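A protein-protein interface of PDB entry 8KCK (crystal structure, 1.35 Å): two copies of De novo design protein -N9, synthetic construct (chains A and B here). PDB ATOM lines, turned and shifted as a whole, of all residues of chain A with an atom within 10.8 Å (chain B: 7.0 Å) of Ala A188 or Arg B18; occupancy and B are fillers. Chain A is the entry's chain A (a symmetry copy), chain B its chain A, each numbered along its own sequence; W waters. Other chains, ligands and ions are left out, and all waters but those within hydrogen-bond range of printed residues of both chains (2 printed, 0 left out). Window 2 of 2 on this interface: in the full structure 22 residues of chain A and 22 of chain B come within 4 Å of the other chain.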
ATOM      1  N   LEU A  29      -1.058   1.729  11.588  1.00  0.00           N
ATOM      2  CA  LEU A  29       0.181   1.052  11.942  1.00  0.00           C
ATOM      3  C   LEU A  29       0.739   1.590  13.260  1.00  0.00           C
ATOM      4  O   LEU A  29       0.767   2.796  13.486  1.00  0.00           O
ATOM      5  CB  LEU A  29       1.252   1.288  10.886  1.00  0.00           C
ATOM      6  CG  LEU A  29       1.012   0.622   9.527  1.00  0.00           C
ATOM      7  CD1 LEU A  29       2.238   0.807   8.616  1.00  0.00           C
ATOM      8  CD2 LEU A  29       0.588  -0.863   9.656  1.00  0.00           C
ATOM      9  N   PRO A  30       1.207   0.721  14.133  1.00  0.00           N
ATOM     10  CA  PRO A  30       1.854   1.170  15.362  1.00  0.00           C
ATOM     11  C   PRO A  30       3.304   1.509  15.128  1.00  0.00           C
ATOM     12  O   PRO A  30       3.974   0.911  14.294  1.00  0.00           O
ATOM     13  CB  PRO A  30       1.757  -0.071  16.267  1.00  0.00           C
ATOM     14  CG  PRO A  30       1.718  -1.305  15.240  1.00  0.00           C
ATOM     15  CD  PRO A  30       0.972  -0.738  14.048  1.00  0.00           C
ATOM     16  N   VAL A  31       3.826   2.401  15.961  1.00  0.00           N
ATOM     17  CA  VAL A  31       5.272   2.547  16.029  1.00  0.00           C
ATOM     18  C   VAL A  31       5.843   1.332  16.757  1.00  0.00           C
ATOM     19  O   VAL A  31       5.445   1.025  17.891  1.00  0.00           O
ATOM     20  CB  VAL A  31       5.651   3.824  16.791  1.00  0.00           C
ATOM     21  CG1 VAL A  31       7.158   3.903  16.973  1.00  0.00           C
ATOM     22  CG2 VAL A  31       5.159   5.084  16.101  1.00  0.00           C
ATOM     23  N   THR A  32       6.755   0.623  16.101  1.00  0.00           N
ATOM     24  CA  THR A  32       7.369  -0.587  16.653  1.00  0.00           C
ATOM     25  C   THR A  32       8.821  -0.582  16.215  1.00  0.00           C
ATOM     26  O   THR A  32       9.204   0.221  15.361  1.00  0.00           O
ATOM     27  CB  THR A  32       6.760  -1.876  16.067  1.00  0.00           C
ATOM     28  OG1 THR A  32       7.026  -1.913  14.663  1.00  0.00           O
ATOM     29  CG2 THR A  32       5.274  -1.993  16.354  1.00  0.00           C
ATOM     30  N   SER A 126       1.583  12.569  17.460  1.00  0.00           N
ATOM     31  CA  SER A 126       2.707  12.694  18.381  1.00  0.00           C
ATOM     32  C   SER A 126       4.001  12.812  17.593  1.00  0.00           C
ATOM     33  O   SER A 126       4.082  12.374  16.429  1.00  0.00           O
ATOM     34  CB  SER A 126       2.800  11.461  19.282  1.00  0.00           C
ATOM     35  OG  SER A 126       3.109  10.287  18.450  1.00  0.00           O
ATOM     36  N   GLU A 128       6.614  11.144  17.996  1.00  0.00           N
ATOM     37  CA  GLU A 128       7.082   9.796  17.740  1.00  0.00           C
ATOM     38  C   GLU A 128       6.347   9.140  16.556  1.00  0.00           C
ATOM     39  O   GLU A 128       6.976   8.513  15.701  1.00  0.00           O
ATOM     40  CB  GLU A 128       6.870   8.972  19.027  1.00  0.00           C
ATOM     41  CG  GLU A 128       7.555   9.471  20.333  1.00  0.00           C
ATOM     42  CD  GLU A 128       7.046  10.768  20.980  1.00  0.00           C
ATOM     43  OE1 GLU A 128       5.863  11.097  20.844  1.00  0.00           O
ATOM     44  OE2 GLU A 128       7.838  11.341  21.771  1.00  0.00           O
ATOM     45  N   GLY A 129       5.021   9.272  16.491  1.00  0.00           N
ATOM     46  CA  GLY A 129       4.302   8.793  15.307  1.00  0.00           C
ATOM     47  C   GLY A 129       4.742   9.547  14.075  1.00  0.00           C
ATOM     48  O   GLY A 129       4.827   8.964  12.983  1.00  0.00           O
ATOM     49  N   ILE A 184      -0.465   6.553  11.898  1.00  0.00           N
ATOM     50  CA  ILE A 184       0.665   6.016  12.652  1.00  0.00           C
ATOM     51  C   ILE A 184       0.541   6.478  14.101  1.00  0.00           C
ATOM     52  O   ILE A 184       0.401   7.684  14.335  1.00  0.00           O
ATOM     53  CB  ILE A 184       2.001   6.485  12.070  1.00  0.00           C
ATOM     54  CG1 ILE A 184       2.155   6.241  10.584  1.00  0.00           C
ATOM     55  CG2 ILE A 184       3.151   5.873  12.869  1.00  0.00           C
ATOM     56  CD1 ILE A 184       2.204   4.792  10.267  1.00  0.00           C
ATOM     57  N   GLY A 185       0.603   5.535  15.030  1.00  0.00           N
ATOM     58  CA  GLY A 185       0.480   5.909  16.429  1.00  0.00           C
ATOM     59  C   GLY A 185       1.500   5.222  17.306  1.00  0.00           C
ATOM     60  O   GLY A 185       1.771   4.013  17.173  1.00  0.00           O
ATOM     61  N   ASP A 186       2.026   6.002  18.263  1.00  0.00           N
ATOM     62  CA  ASP A 186       2.810   5.409  19.348  1.00  0.00           C
ATOM     63  C   ASP A 186       1.818   4.602  20.220  1.00  0.00           C
ATOM     64  O   ASP A 186       0.786   5.169  20.659  1.00  0.00           O
ATOM     65  CB  ASP A 186       3.464   6.570  20.137  1.00  0.00           C
ATOM     66  CG  ASP A 186       4.224   6.050  21.301  1.00  0.00           C
ATOM     67  OD1 ASP A 186       3.574   5.438  22.138  1.00  0.00           O
ATOM     68  OD2 ASP A 186       5.442   6.295  21.368  1.00  0.00           O
ATOM     69  N   PRO A 187       2.095   3.317  20.509  1.00  0.00           N
ATOM     70  CA  PRO A 187       1.056   2.444  21.150  1.00  0.00           C
ATOM     71  C   PRO A 187       0.551   2.913  22.492  1.00  0.00           C
ATOM     72  O   PRO A 187      -0.568   2.557  22.905  1.00  0.00           O
ATOM     73  CB  PRO A 187       1.750   1.083  21.258  1.00  0.00           C
ATOM     74  CG  PRO A 187       2.665   1.029  20.116  1.00  0.00           C
ATOM     75  CD  PRO A 187       3.193   2.511  19.992  1.00  0.00           C
ATOM     76  N   ALA A 188       1.311   3.703  23.184  1.00  0.00           N
ATOM     77  CA  ALA A 188       0.885   4.171  24.490  1.00  0.00           C
ATOM     78  C   ALA A 188       0.198   5.535  24.516  1.00  0.00           C
ATOM     79  O   ALA A 188      -0.328   5.947  25.571  1.00  0.00           O
ATOM     80  CB  ALA A 188       2.139   4.243  25.336  1.00  0.00           C
ATOM     81  N   ASN A 189       0.190   6.267  23.413  1.00  0.00           N
ATOM     82  CA  ASN A 189      -0.151   7.681  23.414  1.00  0.00           C
ATOM     83  C   ASN A 189      -1.650   7.836  23.185  1.00  0.00           C
ATOM     84  O   ASN A 189      -2.148   7.419  22.160  1.00  0.00           O
ATOM     85  CB  ASN A 189       0.663   8.353  22.305  1.00  0.00           C
ATOM     86  CG  ASN A 189       0.443   9.838  22.208  1.00  0.00           C
ATOM     87  OD1 ASN A 189      -0.664  10.313  22.040  1.00  0.00           O
ATOM     88  ND2 ASN A 189       1.519  10.579  22.287  1.00  0.00           N
ATOM     89  N   PRO A 190      -2.415   8.370  24.153  1.00  0.00           N
ATOM     90  CA  PRO A 190      -3.867   8.395  23.962  1.00  0.00           C
ATOM     91  C   PRO A 190      -4.276   9.365  22.904  1.00  0.00           C
ATOM     92  O   PRO A 190      -5.368   9.215  22.351  1.00  0.00           O
ATOM     93  CB  PRO A 190      -4.411   8.836  25.326  1.00  0.00           C
ATOM     94  CG  PRO A 190      -3.333   9.495  25.938  1.00  0.00           C
ATOM     95  CD  PRO A 190      -2.043   8.867  25.481  1.00  0.00           C
ATOM     96  N   THR A 191      -3.470  10.426  22.698  1.00  0.00           N
ATOM     97  CA  THR A 191      -3.762  11.360  21.608  1.00  0.00           C
ATOM     98  C   THR A 191      -3.700  10.638  20.270  1.00  0.00           C
ATOM     99  O   THR A 191      -4.622  10.759  19.458  1.00  0.00           O
ATOM    100  CB  THR A 191      -2.823  12.570  21.604  1.00  0.00           C
ATOM    101  OG1 THR A 191      -2.888  13.243  22.869  1.00  0.00           O
ATOM    102  CG2 THR A 191      -3.238  13.596  20.533  1.00  0.00           C
ATOM    103  N   ASP A 192      -2.624   9.884  20.028  1.00  0.00           N
ATOM    104  CA  ASP A 192      -2.561   9.103  18.796  1.00  0.00           C
ATOM    105  C   ASP A 192      -3.738   8.137  18.718  1.00  0.00           C
ATOM    106  O   ASP A 192      -4.345   7.987  17.650  1.00  0.00           O
ATOM    107  CB  ASP A 192      -1.260   8.301  18.711  1.00  0.00           C
ATOM    108  CG  ASP A 192      -0.031   9.161  18.382  1.00  0.00           C
ATOM    109  OD1 ASP A 192      -0.188  10.254  17.855  1.00  0.00           O
ATOM    110  OD2 ASP A 192       1.085   8.647  18.560  1.00  0.00           O
ATOM    111  N   ALA A 193      -4.093   7.496  19.837  1.00  0.00           N
ATOM    112  CA  ALA A 193      -5.229   6.575  19.817  1.00  0.00           C
ATOM    113  C   ALA A 193      -6.529   7.302  19.538  1.00  0.00           C
ATOM    114  O   ALA A 193      -7.397   6.779  18.818  1.00  0.00           O
ATOM    115  CB  ALA A 193      -5.306   5.791  21.124  1.00  0.00           C
ATOM    116  N   ALA A 194      -6.690   8.491  20.128  1.00  0.00           N
ATOM    117  CA  ALA A 194      -7.881   9.266  19.866  1.00  0.00           C
ATOM    118  C   ALA A 194      -7.962   9.646  18.395  1.00  0.00           C
ATOM    119  O   ALA A 194      -9.040   9.604  17.807  1.00  0.00           O
ATOM    120  CB  ALA A 194      -7.929  10.492  20.780  1.00  0.00           C
ATOM    121  N   LEU A 195      -6.834  10.014  17.779  1.00  0.00           N
ATOM    122  CA  LEU A 195      -6.888  10.368  16.365  1.00  0.00           C
ATOM    123  C   LEU A 195      -7.297   9.161  15.527  1.00  0.00           C
ATOM    124  O   LEU A 195      -8.136   9.274  14.635  1.00  0.00           O
ATOM    125  CB  LEU A 195      -5.529  10.877  15.905  1.00  0.00           C
ATOM    126  CG  LEU A 195      -5.389  11.239  14.428  1.00  0.00           C
ATOM    127  CD1 LEU A 195      -6.416  12.277  14.046  1.00  0.00           C
ATOM    128  CD2 LEU A 195      -3.992  11.763  14.198  1.00  0.00           C
ATOM    129  N   GLU B  13      -9.267  -5.486  29.276  1.00  0.00           N
ATOM    130  CA  GLU B  13      -8.192  -6.430  28.989  1.00  0.00           C
ATOM    131  C   GLU B  13      -6.980  -5.728  28.399  1.00  0.00           C
ATOM    132  O   GLU B  13      -5.845  -6.121  28.702  1.00  0.00           O
ATOM    133  CB  GLU B  13      -8.673  -7.583  28.062  1.00  0.00           C
ATOM    134  CG  GLU B  13      -9.722  -8.480  28.729  1.00  0.00           C
ATOM    135  CD  GLU B  13      -9.200  -9.303  29.929  1.00  0.00           C
ATOM    136  OE1 GLU B  13      -7.975  -9.511  30.043  1.00  0.00           O
ATOM    137  OE2 GLU B  13     -10.044  -9.755  30.721  1.00  0.00           O
ATOM    138  N   LEU B  14      -7.188  -4.689  27.594  1.00  0.00           N
ATOM    139  CA  LEU B  14      -6.048  -3.909  27.096  1.00  0.00           C
ATOM    140  C   LEU B  14      -5.300  -3.259  28.251  1.00  0.00           C
ATOM    141  O   LEU B  14      -4.058  -3.284  28.324  1.00  0.00           O
ATOM    142  CB  LEU B  14      -6.549  -2.847  26.136  1.00  0.00           C
ATOM    143  CG  LEU B  14      -7.079  -3.343  24.800  1.00  0.00           C
ATOM    144  CD1 LEU B  14      -7.775  -2.202  24.105  1.00  0.00           C
ATOM    145  CD2 LEU B  14      -5.926  -3.886  23.891  1.00  0.00           C
ATOM    146  N   ARG B  15      -6.042  -2.646  29.175  1.00  0.00           N
ATOM    147  CA  ARG B  15      -5.410  -2.018  30.340  1.00  0.00           C
ATOM    148  C   ARG B  15      -4.652  -3.062  31.140  1.00  0.00           C
ATOM    149  O   ARG B  15      -3.534  -2.804  31.617  1.00  0.00           O
ATOM    150  CB  ARG B  15      -6.506  -1.432  31.207  1.00  0.00           C
ATOM    151  CG  ARG B  15      -6.889  -0.075  30.778  1.00  0.00           C
ATOM    152  CD  ARG B  15      -7.761   0.539  31.871  1.00  0.00           C
ATOM    153  NE  ARG B  15      -8.318   1.804  31.427  1.00  0.00           N
ATOM    154  CZ  ARG B  15      -7.627   2.934  31.436  1.00  0.00           C
ATOM    155  NH1 ARG B  15      -6.369   2.967  31.851  1.00  0.00           N
ATOM    156  NH2 ARG B  15      -8.198   4.050  30.989  1.00  0.00           N
ATOM    157  N   ALA B  16      -5.246  -4.244  31.335  1.00  0.00           N
ATOM    158  CA  ALA B  16      -4.616  -5.257  32.159  1.00  0.00           C
ATOM    159  C   ALA B  16      -3.348  -5.785  31.514  1.00  0.00           C
ATOM    160  O   ALA B  16      -2.382  -6.120  32.200  1.00  0.00           O
ATOM    161  CB  ALA B  16      -5.594  -6.390  32.449  1.00  0.00           C
ATOM    162  N   PHE B  17      -3.342  -5.938  30.182  1.00  0.00           N
ATOM    163  CA  PHE B  17      -2.126  -6.421  29.537  1.00  0.00           C
ATOM    164  C   PHE B  17      -0.976  -5.460  29.739  1.00  0.00           C
ATOM    165  O   PHE B  17       0.164  -5.885  29.987  1.00  0.00           O
ATOM    166  CB  PHE B  17      -2.378  -6.687  28.032  1.00  0.00           C
ATOM    167  CG  PHE B  17      -1.262  -7.446  27.345  1.00  0.00           C
ATOM    168  CD1 PHE B  17      -0.165  -6.770  26.819  1.00  0.00           C
ATOM    169  CD2 PHE B  17      -1.319  -8.828  27.243  1.00  0.00           C
ATOM    170  CE1 PHE B  17       0.843  -7.485  26.185  1.00  0.00           C
ATOM    171  CE2 PHE B  17      -0.298  -9.567  26.659  1.00  0.00           C
ATOM    172  CZ  PHE B  17       0.816  -8.879  26.141  1.00  0.00           C
ATOM    173  N   ARG B  18      -1.254  -4.184  29.562  1.00  0.00           N
ATOM    174  CA  ARG B  18      -0.220  -3.172  29.772  1.00  0.00           C
ATOM    175  C   ARG B  18       0.236  -3.106  31.225  1.00  0.00           C
ATOM    176  O   ARG B  18       1.440  -2.924  31.498  1.00  0.00           O
ATOM    177  CB  ARG B  18      -0.749  -1.809  29.310  1.00  0.00           C
ATOM    178  CG  ARG B  18      -0.870  -1.701  27.795  1.00  0.00           C
ATOM    179  CD  ARG B  18      -1.245  -0.300  27.292  1.00  0.00           C
ATOM    180  NE  ARG B  18      -0.335   0.760  27.712  1.00  0.00           N
ATOM    181  CZ  ARG B  18       0.861   1.011  27.216  1.00  0.00           C
ATOM    182  NH1 ARG B  18       1.334   0.336  26.155  1.00  0.00           N
ATOM    183  NH2 ARG B  18       1.607   1.944  27.786  1.00  0.00           N
ATOM    184  N   ALA B  19      -0.700  -3.195  32.177  1.00  0.00           N
ATOM    185  CA  ALA B  19      -0.318  -3.141  33.591  1.00  0.00           C
ATOM    186  C   ALA B  19       0.566  -4.323  33.953  1.00  0.00           C
ATOM    187  O   ALA B  19       1.342  -4.256  34.918  1.00  0.00           O
ATOM    188  CB  ALA B  19      -1.565  -3.174  34.472  1.00  0.00           C
ATOM    189  N   ALA B  20       0.397  -5.453  33.274  1.00  0.00           N
ATOM    190  CA  ALA B  20       1.249  -6.599  33.504  1.00  0.00           C
ATOM    191  C   ALA B  20       2.634  -6.485  32.873  1.00  0.00           C
ATOM    192  O   ALA B  20       3.475  -7.354  33.102  1.00  0.00           O
ATOM    193  CB  ALA B  20       0.525  -7.891  33.095  1.00  0.00           C
ATOM    194  N   GLY B  21       2.903  -5.455  32.074  1.00  0.00           N
ATOM    195  CA  GLY B  21       4.228  -5.210  31.566  1.00  0.00           C
ATOM    196  C   GLY B  21       4.425  -5.377  30.076  1.00  0.00           C
ATOM    197  O   GLY B  21       5.564  -5.313  29.605  1.00  0.00           O
ATOM    198  N   GLY B  22       3.356  -5.556  29.280  1.00  0.00           N
ATOM    199  CA  GLY B  22       3.500  -5.759  27.850  1.00  0.00           C
ATOM    200  C   GLY B  22       2.817  -4.666  27.062  1.00  0.00           C
ATOM    201  O   GLY B  22       1.812  -4.102  27.489  1.00  0.00           O
ATOM    202  N   THR B  23       3.367  -4.391  25.896  1.00  0.00           N
ATOM    203  CA  THR B  23       2.742  -3.441  24.963  1.00  0.00           C
ATOM    204  C   THR B  23       1.692  -4.180  24.100  1.00  0.00           C
ATOM    205  O   THR B  23       1.928  -5.286  23.621  1.00  0.00           O
ATOM    206  CB  THR B  23       3.806  -2.833  24.052  1.00  0.00           C
ATOM    207  OG1 THR B  23       4.637  -2.028  24.863  1.00  0.00           O
ATOM    208  CG2 THR B  23       3.156  -1.938  22.986  1.00  0.00           C
ATOM    209  N   VAL B  24       0.532  -3.544  23.894  1.00  0.00           N
ATOM    210  CA  VAL B  24      -0.430  -3.968  22.875  1.00  0.00           C
ATOM    211  C   VAL B  24      -0.165  -3.176  21.601  1.00  0.00           C
ATOM    212  O   VAL B  24      -0.217  -1.955  21.605  1.00  0.00           O
ATOM    213  CB  VAL B  24      -1.899  -3.782  23.290  1.00  0.00           C
ATOM    214  CG1 VAL B  24      -2.798  -4.346  22.153  1.00  0.00           C
ATOM    215  CG2 VAL B  24      -2.223  -4.525  24.630  1.00  0.00           C
ATOM    216  N   ARG B 169      -2.407 -12.391  27.990  1.00  0.00           N
ATOM    217  CA  ARG B 169      -1.872 -11.946  29.265  1.00  0.00           C
ATOM    218  C   ARG B 169      -1.442 -13.138  30.105  1.00  0.00           C
ATOM    219  O   ARG B 169      -0.363 -13.134  30.720  1.00  0.00           O
ATOM    220  CB  ARG B 169      -2.945 -11.135  30.001  1.00  0.00           C
ATOM    221  CG  ARG B 169      -2.528 -10.629  31.419  1.00  0.00           C
ATOM    222  CD  ARG B 169      -3.436  -9.548  31.921  1.00  0.00           C
ATOM    223  NE  ARG B 169      -4.849  -9.884  31.766  1.00  0.00           N
ATOM    224  CZ  ARG B 169      -5.537 -10.629  32.613  1.00  0.00           C
ATOM    225  NH1 ARG B 169      -4.985 -11.081  33.735  1.00  0.00           N
ATOM    226  NH2 ARG B 169      -6.801 -10.939  32.319  1.00  0.00           N
ATOM    227  N   TYR B 203      -9.693   0.955  22.390  1.00  0.00           N
ATOM    228  CA  TYR B 203      -8.288   1.119  22.663  1.00  0.00           C
ATOM    229  C   TYR B 203      -7.986   2.537  23.171  1.00  0.00           C
ATOM    230  O   TYR B 203      -7.181   2.731  24.098  1.00  0.00           O
ATOM    231  CB  TYR B 203      -7.533   0.807  21.356  1.00  0.00           C
ATOM    232  CG  TYR B 203      -6.068   0.850  21.441  1.00  0.00           C
ATOM    233  CD1 TYR B 203      -5.358  -0.270  21.864  1.00  0.00           C
ATOM    234  CD2 TYR B 203      -5.374   1.960  21.045  1.00  0.00           C
ATOM    235  CE1 TYR B 203      -4.005  -0.292  21.904  1.00  0.00           C
ATOM    236  CE2 TYR B 203      -4.001   1.960  21.077  1.00  0.00           C
ATOM    237  CZ  TYR B 203      -3.339   0.829  21.532  1.00  0.00           C
ATOM    238  OH  TYR B 203      -1.949   0.891  21.526  1.00  0.00           O
ATOM    239  N   ALA B 206      -8.687   2.721  26.775  1.00  0.00           N
ATOM    240  CA  ALA B 206      -7.742   2.022  27.619  1.00  0.00           C
ATOM    241  C   ALA B 206      -6.506   2.853  27.917  1.00  0.00           C
ATOM    242  O   ALA B 206      -5.849   2.614  28.928  1.00  0.00           O
ATOM    243  CB  ALA B 206      -7.354   0.694  26.926  1.00  0.00           C
ATOM    244  N   LEU B 207      -6.154   3.791  27.030  1.00  0.00           N
ATOM    245  CA  LEU B 207      -4.945   4.600  27.158  1.00  0.00           C
ATOM    246  C   LEU B 207      -5.173   5.902  27.896  1.00  0.00           C
ATOM    247  O   LEU B 207      -4.195   6.554  28.271  1.00  0.00           O
ATOM    248  CB  LEU B 207      -4.437   4.907  25.750  1.00  0.00           C
ATOM    249  CG  LEU B 207      -3.948   3.721  24.929  1.00  0.00           C
ATOM    250  CD1 LEU B 207      -3.249   4.265  23.676  1.00  0.00           C
ATOM    251  CD2 LEU B 207      -3.014   2.818  25.730  1.00  0.00           C
ATOM    252  N   GLU B 208      -6.420   6.301  28.114  1.00  0.00           N
ATOM    253  CA  GLU B 208      -6.722   7.589  28.728  1.00  0.00           C
ATOM    254  C   GLU B 208      -6.173   7.574  30.135  1.00  0.00           C
ATOM    255  O   GLU B 208      -6.231   6.539  30.788  1.00  0.00           O
ATOM    256  CB  GLU B 208      -8.225   7.722  28.808  1.00  0.00           C
ATOM    257  CG  GLU B 208      -8.849   8.331  27.576  1.00  0.00           C
ATOM    258  CD  GLU B 208     -10.291   8.752  27.812  1.00  0.00           C
ATOM    259  OE1 GLU B 208     -11.013   8.965  26.810  1.00  0.00           O
ATOM    260  OE2 GLU B 208     -10.688   8.898  28.996  1.00  0.00           O
HETATM  261  O   HOH W   1      -1.435   5.354  27.990  1.00  0.00           O
HETATM  262  O   HOH W   2      -0.334  -0.534  24.062  1.00  0.00           O
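Ala A188 touches two residues of chain B. Arg B18 touches just one residue of chain A: Ala A188 (3.4 Å). No residue of chain A comes within 4 Å of Phe B17. No residue of chain A comes within 4 Å of Ala B19. No residue of chain A comes within 4 Å of Ala B20. No residue of chain A comes within 4 Å of Gly B22. Val B24 touches one residue of chain A. Leu B207 touches just these residues of chain A: Pro A187 (3.3 Å), Ala A188 (3.8 Å), Asn A189 (3.7 Å), Pro A190 (3.7 Å) and Ala A193 (3.6 Å). Of the printed residues of chain B, Asn A189 touches Leu B207 (3.7 Å). Printed residues of chain B within 4 Å of Pro A187: Thr B23, Val B24, Tyr B203 and Leu B207. Of the printed residues of chain A, Tyr B203 touches Pro A187 and Ala A193. Printed residues of chain B within 4 Å of Pro A190: Leu B207 (3.7 Å). Of the printed residues of chain B, Ala A193 touches Tyr B203 (3.8 Å) and Leu B207 (3.6 Å). Glu A128 touches none of the printed residues of chain B. Thr A32 touches none of the printed residues of chain B. The nearest residue of chain A that does not touch Arg B18 is Pro A187 (4.4 Å). The nearest printed residue of chain B that does not touch Ala A193 is Glu B208 (7.1 Å).
The backbone carbonyl oxygen (O) of Val B24 lies within hydrogen-bond range of the side-chain hydroxyl (OH) of Tyr B203 (3.3 Å). OD1 of Asp A186 lies within hydrogen-bond range of N of Ala A188 (3.0 Å). The backbone NH (N) of Thr A191 sits at hydrogen-bond distance from the side-chain amide oxygen (OD1) of Asn A189 (2.9 Å). The side-chain amide oxygen (OD1) of Asn A189 lies within hydrogen-bond range of the backbone NH (N) of Asp A192 (2.8 Å).
Printed residues of chain B that touch a printed residue of chain A: Arg B18, Thr B23, Val B24, Tyr B203 and Leu B207. Hydrophobic or aromatic side chains of chain A within 4 Å of the printed part of chain B: Pro A187, Ala A188, Pro A190 and Ala A193. Along chain A the printed residues that touch a printed residue of chain B span positions 187 to 193. Among the printed residues, 10 pairs touch across the chains. Among the printed residues, no Asp or Glu carboxylate lies within 4 Å of a Lys or Arg side-chain nitrogen of the other chain.
Water W1 bridges O of Ala A188 and O of Leu B207. Water W2 lies within hydrogen-bond range of the guanidinium group (NH1) of Arg B18 (2.8 Å), the backbone carbonyl oxygen (O) of Val B24 (2.8 Å), the backbone carbonyl oxygen (O) of Pro A187 (3.3 Å) and the side-chain hydroxyl (OH) of Tyr B203 (3.3 Å).
O of Pro A187 sits at hydrogen-bond distance from OH of Tyr B203 (2.6 Å).
No position is printed for both chains. Of the 10 pairs that touch across the chains among the printed residues, none has its exchanged pair printed and touching as well.
Thr B23 touches Pro A187 (CG2 to CB, 3.8 Å). Val B24 touches Pro A187. Pro A187 touches Leu B207 (O to CD1, 3.3 Å). Ala A188 touches Arg B18 (CB to NH2, 3.4 Å). Leu B207 touches Ala A188 (CD1 to C, 3.8 Å). Leu B207 touches Asn A189. CB of Pro A190 touches O of Leu B207 (3.7 Å). CD2 of Tyr B203 touches CB of Ala A193, 3.8 Å away. Ala A193 touches Leu B207.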
